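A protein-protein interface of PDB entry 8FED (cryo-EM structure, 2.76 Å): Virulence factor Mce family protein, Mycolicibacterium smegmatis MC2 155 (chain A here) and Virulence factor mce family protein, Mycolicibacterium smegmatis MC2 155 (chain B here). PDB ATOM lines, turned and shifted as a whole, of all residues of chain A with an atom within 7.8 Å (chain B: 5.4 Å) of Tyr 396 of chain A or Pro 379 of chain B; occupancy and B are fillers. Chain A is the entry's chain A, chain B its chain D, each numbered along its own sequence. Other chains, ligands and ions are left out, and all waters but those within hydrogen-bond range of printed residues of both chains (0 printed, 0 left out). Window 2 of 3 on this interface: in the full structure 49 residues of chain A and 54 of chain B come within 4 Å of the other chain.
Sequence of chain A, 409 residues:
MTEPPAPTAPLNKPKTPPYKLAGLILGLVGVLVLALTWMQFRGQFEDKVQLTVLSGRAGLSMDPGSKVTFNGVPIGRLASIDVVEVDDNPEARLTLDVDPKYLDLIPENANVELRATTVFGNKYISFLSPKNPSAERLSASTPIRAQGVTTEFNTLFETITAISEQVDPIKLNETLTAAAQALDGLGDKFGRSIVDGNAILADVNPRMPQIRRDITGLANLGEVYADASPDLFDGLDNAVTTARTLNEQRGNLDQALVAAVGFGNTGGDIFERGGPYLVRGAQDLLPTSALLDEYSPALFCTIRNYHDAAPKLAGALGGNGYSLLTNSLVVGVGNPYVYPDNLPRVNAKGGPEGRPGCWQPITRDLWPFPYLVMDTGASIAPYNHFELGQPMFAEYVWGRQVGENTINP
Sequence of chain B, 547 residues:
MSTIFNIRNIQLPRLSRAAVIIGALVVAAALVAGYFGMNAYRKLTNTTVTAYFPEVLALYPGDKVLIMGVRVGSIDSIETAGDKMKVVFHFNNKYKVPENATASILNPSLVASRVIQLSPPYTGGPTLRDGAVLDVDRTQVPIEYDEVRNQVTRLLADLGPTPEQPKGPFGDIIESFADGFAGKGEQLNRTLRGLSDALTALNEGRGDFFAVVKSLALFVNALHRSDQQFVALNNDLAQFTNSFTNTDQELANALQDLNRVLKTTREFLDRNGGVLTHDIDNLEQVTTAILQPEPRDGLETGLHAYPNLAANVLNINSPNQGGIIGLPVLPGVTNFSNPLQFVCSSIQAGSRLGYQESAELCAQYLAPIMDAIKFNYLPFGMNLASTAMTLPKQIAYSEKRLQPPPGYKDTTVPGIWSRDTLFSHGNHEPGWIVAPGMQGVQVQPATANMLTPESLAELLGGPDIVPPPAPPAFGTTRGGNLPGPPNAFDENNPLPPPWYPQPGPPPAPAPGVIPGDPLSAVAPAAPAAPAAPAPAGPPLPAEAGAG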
ATOM      1  N   PRO A 391     -27.367  -8.902  25.813  1.00  0.00           N
ATOM      2  CA  PRO A 391     -26.035  -8.257  25.832  1.00  0.00           C
ATOM      3  C   PRO A 391     -26.160  -6.755  26.072  1.00  0.00           C
ATOM      4  O   PRO A 391     -25.908  -5.924  25.189  1.00  0.00           O
ATOM      5  CB  PRO A 391     -25.480  -8.588  24.441  1.00  0.00           C
ATOM      6  CG  PRO A 391     -26.487  -9.500  23.784  1.00  0.00           C
ATOM      7  CD  PRO A 391     -27.781  -9.182  24.431  1.00  0.00           C
ATOM      8  N   PHE A 393     -24.474  -4.633  28.013  1.00  0.00           N
ATOM      9  CA  PHE A 393     -23.194  -3.945  27.919  1.00  0.00           C
ATOM     10  C   PHE A 393     -22.174  -4.918  27.353  1.00  0.00           C
ATOM     11  O   PHE A 393     -22.079  -6.058  27.817  1.00  0.00           O
ATOM     12  CB  PHE A 393     -22.744  -3.419  29.289  1.00  0.00           C
ATOM     13  CG  PHE A 393     -21.340  -2.872  29.304  1.00  0.00           C
ATOM     14  CD1 PHE A 393     -21.075  -1.596  28.837  1.00  0.00           C
ATOM     15  CD2 PHE A 393     -20.291  -3.628  29.803  1.00  0.00           C
ATOM     16  CE1 PHE A 393     -19.790  -1.089  28.857  1.00  0.00           C
ATOM     17  CE2 PHE A 393     -19.004  -3.126  29.822  1.00  0.00           C
ATOM     18  CZ  PHE A 393     -18.753  -1.856  29.349  1.00  0.00           C
ATOM     19  N   ALA A 394     -21.421  -4.474  26.351  1.00  0.00           N
ATOM     20  CA  ALA A 394     -20.422  -5.311  25.706  1.00  0.00           C
ATOM     21  C   ALA A 394     -19.116  -4.546  25.584  1.00  0.00           C
ATOM     22  O   ALA A 394     -19.112  -3.346  25.298  1.00  0.00           O
ATOM     23  CB  ALA A 394     -20.890  -5.777  24.322  1.00  0.00           C
ATOM     24  N   GLU A 395     -18.009  -5.248  25.805  1.00  0.00           N
ATOM     25  CA  GLU A 395     -16.674  -4.685  25.674  1.00  0.00           C
ATOM     26  C   GLU A 395     -15.961  -5.352  24.506  1.00  0.00           C
ATOM     27  O   GLU A 395     -15.968  -6.582  24.390  1.00  0.00           O
ATOM     28  CB  GLU A 395     -15.875  -4.873  26.965  1.00  0.00           C
ATOM     29  CG  GLU A 395     -14.561  -4.116  27.001  1.00  0.00           C
ATOM     30  CD  GLU A 395     -13.838  -4.273  28.324  1.00  0.00           C
ATOM     31  OE1 GLU A 395     -14.328  -5.035  29.185  1.00  0.00           O
ATOM     32  OE2 GLU A 395     -12.781  -3.633  28.506  1.00  0.00           O
ATOM     33  N   TYR A 396     -15.351  -4.540  23.644  1.00  0.00           N
ATOM     34  CA  TYR A 396     -14.726  -5.023  22.422  1.00  0.00           C
ATOM     35  C   TYR A 396     -13.207  -5.068  22.525  1.00  0.00           C
ATOM     36  O   TYR A 396     -12.521  -5.085  21.497  1.00  0.00           O
ATOM     37  CB  TYR A 396     -15.158  -4.162  21.233  1.00  0.00           C
ATOM     38  CG  TYR A 396     -16.650  -4.175  20.993  1.00  0.00           C
ATOM     39  CD1 TYR A 396     -17.410  -5.298  21.297  1.00  0.00           C
ATOM     40  CD2 TYR A 396     -17.302  -3.062  20.485  1.00  0.00           C
ATOM     41  CE1 TYR A 396     -18.774  -5.318  21.088  1.00  0.00           C
ATOM     42  CE2 TYR A 396     -18.667  -3.070  20.274  1.00  0.00           C
ATOM     43  CZ  TYR A 396     -19.397  -4.202  20.577  1.00  0.00           C
ATOM     44  OH  TYR A 396     -20.757  -4.219  20.369  1.00  0.00           O
ATOM     45  N   VAL A 397     -12.669  -5.089  23.739  1.00  0.00           N
ATOM     46  CA  VAL A 397     -11.237  -5.244  23.959  1.00  0.00           C
ATOM     47  C   VAL A 397     -10.877  -6.683  24.299  1.00  0.00           C
ATOM     48  O   VAL A 397      -9.976  -7.264  23.695  1.00  0.00           O
ATOM     49  CB  VAL A 397     -10.756  -4.273  25.059  1.00  0.00           C
ATOM     50  CG1 VAL A 397      -9.238  -4.241  25.102  1.00  0.00           C
ATOM     51  CG2 VAL A 397     -11.319  -2.883  24.822  1.00  0.00           C
ATOM     52  N   TRP A 398     -11.573  -7.277  25.267  1.00  0.00           N
ATOM     53  CA  TRP A 398     -11.366  -8.670  25.635  1.00  0.00           C
ATOM     54  C   TRP A 398     -12.578  -9.543  25.338  1.00  0.00           C
ATOM     55  O   TRP A 398     -12.601 -10.712  25.737  1.00  0.00           O
ATOM     56  CB  TRP A 398     -10.987  -8.779  27.114  1.00  0.00           C
ATOM     57  CG  TRP A 398      -9.565  -8.398  27.385  1.00  0.00           C
ATOM     58  CD1 TRP A 398      -8.462  -9.187  27.234  1.00  0.00           C
ATOM     59  CD2 TRP A 398      -9.089  -7.131  27.854  1.00  0.00           C
ATOM     60  NE1 TRP A 398      -7.330  -8.490  27.578  1.00  0.00           N
ATOM     61  CE2 TRP A 398      -7.688  -7.225  27.964  1.00  0.00           C
ATOM     62  CE3 TRP A 398      -9.712  -5.927  28.195  1.00  0.00           C
ATOM     63  CZ2 TRP A 398      -6.900  -6.161  28.397  1.00  0.00           C
ATOM     64  CZ3 TRP A 398      -8.928  -4.872  28.624  1.00  0.00           C
ATOM     65  CH2 TRP A 398      -7.538  -4.996  28.721  1.00  0.00           C
ATOM     66  N   GLY A 399     -13.578  -9.009  24.643  1.00  0.00           N
ATOM     67  CA  GLY A 399     -14.722  -9.804  24.223  1.00  0.00           C
ATOM     68  C   GLY A 399     -15.548 -10.361  25.361  1.00  0.00           C
ATOM     69  O   GLY A 399     -15.986 -11.516  25.301  1.00  0.00           O
ATOM     70  N   ARG A 400     -15.776  -9.563  26.399  1.00  0.00           N
ATOM     71  CA  ARG A 400     -16.579  -9.964  27.545  1.00  0.00           C
ATOM     72  C   ARG A 400     -17.747  -9.001  27.684  1.00  0.00           C
ATOM     73  O   ARG A 400     -17.552  -7.781  27.691  1.00  0.00           O
ATOM     74  CB  ARG A 400     -15.741  -9.987  28.826  1.00  0.00           C
ATOM     75  CG  ARG A 400     -16.391 -10.725  29.984  1.00  0.00           C
ATOM     76  CD  ARG A 400     -15.344 -11.252  30.950  1.00  0.00           C
ATOM     77  NE  ARG A 400     -14.391 -10.218  31.335  1.00  0.00           N
ATOM     78  CZ  ARG A 400     -13.299 -10.437  32.054  1.00  0.00           C
ATOM     79  NH1 ARG A 400     -12.986 -11.648  32.486  1.00  0.00           N
ATOM     80  NH2 ARG A 400     -12.500  -9.415  32.347  1.00  0.00           N
ATOM     81  N   GLN A 401     -18.953  -9.548  27.793  1.00  0.00           N
ATOM     82  CA  GLN A 401     -20.171  -8.754  27.810  1.00  0.00           C
ATOM     83  C   GLN A 401     -21.065  -9.190  28.961  1.00  0.00           C
ATOM     84  O   GLN A 401     -20.993 -10.328  29.432  1.00  0.00           O
ATOM     85  CB  GLN A 401     -20.921  -8.860  26.467  1.00  0.00           C
ATOM     86  CG  GLN A 401     -20.824 -10.221  25.779  1.00  0.00           C
ATOM     87  CD  GLN A 401     -21.817 -11.236  26.308  1.00  0.00           C
ATOM     88  OE1 GLN A 401     -22.687 -10.911  27.112  1.00  0.00           O
ATOM     89  NE2 GLN A 401     -21.693 -12.476  25.852  1.00  0.00           N
ATOM     90  N   TYR B 377     -14.164   1.944  15.389  1.00  0.00           N
ATOM     91  CA  TYR B 377     -15.382   2.296  16.117  1.00  0.00           C
ATOM     92  C   TYR B 377     -15.079   2.276  17.612  1.00  0.00           C
ATOM     93  O   TYR B 377     -13.965   1.958  18.039  1.00  0.00           O
ATOM     94  CB  TYR B 377     -16.541   1.361  15.762  1.00  0.00           C
ATOM     95  CG  TYR B 377     -16.242  -0.111  15.923  1.00  0.00           C
ATOM     96  CD1 TYR B 377     -15.731  -0.854  14.867  1.00  0.00           C
ATOM     97  CD2 TYR B 377     -16.492  -0.763  17.119  1.00  0.00           C
ATOM     98  CE1 TYR B 377     -15.465  -2.198  15.006  1.00  0.00           C
ATOM     99  CE2 TYR B 377     -16.229  -2.105  17.268  1.00  0.00           C
ATOM    100  CZ  TYR B 377     -15.717  -2.820  16.209  1.00  0.00           C
ATOM    101  OH  TYR B 377     -15.455  -4.161  16.358  1.00  0.00           O
ATOM    102  N   LEU B 378     -16.092   2.619  18.405  1.00  0.00           N
ATOM    103  CA  LEU B 378     -15.913   2.755  19.843  1.00  0.00           C
ATOM    104  C   LEU B 378     -15.714   1.389  20.496  1.00  0.00           C
ATOM    105  O   LEU B 378     -16.333   0.404  20.084  1.00  0.00           O
ATOM    106  CB  LEU B 378     -17.121   3.453  20.466  1.00  0.00           C
ATOM    107  CG  LEU B 378     -17.411   4.878  19.994  1.00  0.00           C
ATOM    108  CD1 LEU B 378     -18.682   5.398  20.638  1.00  0.00           C
ATOM    109  CD2 LEU B 378     -16.239   5.791  20.305  1.00  0.00           C
ATOM    110  N   PRO B 379     -14.859   1.300  21.521  1.00  0.00           N
ATOM    111  CA  PRO B 379     -14.634   0.006  22.187  1.00  0.00           C
ATOM    112  C   PRO B 379     -15.843  -0.522  22.934  1.00  0.00           C
ATOM    113  O   PRO B 379     -15.887  -1.722  23.228  1.00  0.00           O
ATOM    114  CB  PRO B 379     -13.477   0.301  23.153  1.00  0.00           C
ATOM    115  CG  PRO B 379     -12.872   1.584  22.668  1.00  0.00           C
ATOM    116  CD  PRO B 379     -13.994   2.358  22.066  1.00  0.00           C
ATOM    117  N   PHE B 380     -16.816   0.323  23.260  1.00  0.00           N
ATOM    118  CA  PHE B 380     -17.940  -0.056  24.106  1.00  0.00           C
ATOM    119  C   PHE B 380     -19.251   0.142  23.361  1.00  0.00           C
ATOM    120  O   PHE B 380     -19.408   1.104  22.602  1.00  0.00           O
ATOM    121  CB  PHE B 380     -17.942   0.754  25.407  1.00  0.00           C
ATOM    122  CG  PHE B 380     -17.512   2.185  25.235  1.00  0.00           C
ATOM    123  CD1 PHE B 380     -18.387   3.137  24.741  1.00  0.00           C
ATOM    124  CD2 PHE B 380     -16.228   2.580  25.576  1.00  0.00           C
ATOM    125  CE1 PHE B 380     -17.992   4.451  24.586  1.00  0.00           C
ATOM    126  CE2 PHE B 380     -15.828   3.895  25.424  1.00  0.00           C
ATOM    127  CZ  PHE B 380     -16.712   4.830  24.928  1.00  0.00           C
ATOM    128  N   GLY B 381     -20.185  -0.772  23.579  1.00  0.00           N
ATOM    129  CA  GLY B 381     -21.495  -0.681  22.964  1.00  0.00           C
ATOM    130  C   GLY B 381     -22.571  -1.112  23.935  1.00  0.00           C
ATOM    131  O   GLY B 381     -22.341  -1.935  24.823  1.00  0.00           O
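Of chain B, only Tyr 377 (3.5 Å), Leu 378 (3.6 Å) and Pro 379 (2.9 Å) come within 4 Å of Tyr 396 of chain A. Pro 379 of chain B touches just these residues of chain A: Glu 395 (3.8 Å) and Tyr 396 (2.9 Å). Printed residues of chain A within 4 Å of Tyr 377 of chain B: Tyr 396. Of the printed residues of chain B, Ala 394 of chain A touches Phe 380 (3.7 Å) and Gly 381 (3.1 Å). Printed residues of chain A within 4 Å of Phe 380 of chain B: Ala 394. Of the printed residues of chain A, Leu 378 of chain B touches Tyr 396 (3.6 Å). The nearest residue of chain B that does not touch Tyr 396 of chain A is Gly 381 of chain B (4.3 Å).
Among the printed residues, merely in contact across the chains: Tyr 396 of chain A with Tyr 377 of chain B (3.5 Å), Tyr 396 of chain A with Leu 378 of chain B (3.6 Å), Ala 394 of chain A with Phe 380 of chain B (3.7 Å), Phe 393 of chain A with Gly 381 of chain B (3.8 Å) and Glu 395 of chain A with Pro 379 of chain B (3.8 Å).
Of the 10 printed residues of chain A, 4 touch a printed residue of chain B. Printed residues of chain A that touch a printed residue of chain B: Phe 393, Ala 394, Glu 395 and Tyr 396. Among the printed residues, 7 pairs touch across the chains. Among the printed residues, no Asp or Glu carboxylate lies within 4 Å of a Lys or Arg side-chain nitrogen of the other chain.
The backbone NH (N) of Glu 395 of chain A sits at hydrogen-bond distance from the backbone carbonyl oxygen (O) of Arg 400 of chain A.
The backbone NH (N) of Ala 394 of chain A sits at hydrogen-bond distance from the backbone carbonyl oxygen (O) of Gly 381 of chain B, 3.1 Å away. N of Tyr 396 of chain A is in hydrogen-bond range of O of Pro 379 of chain B.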
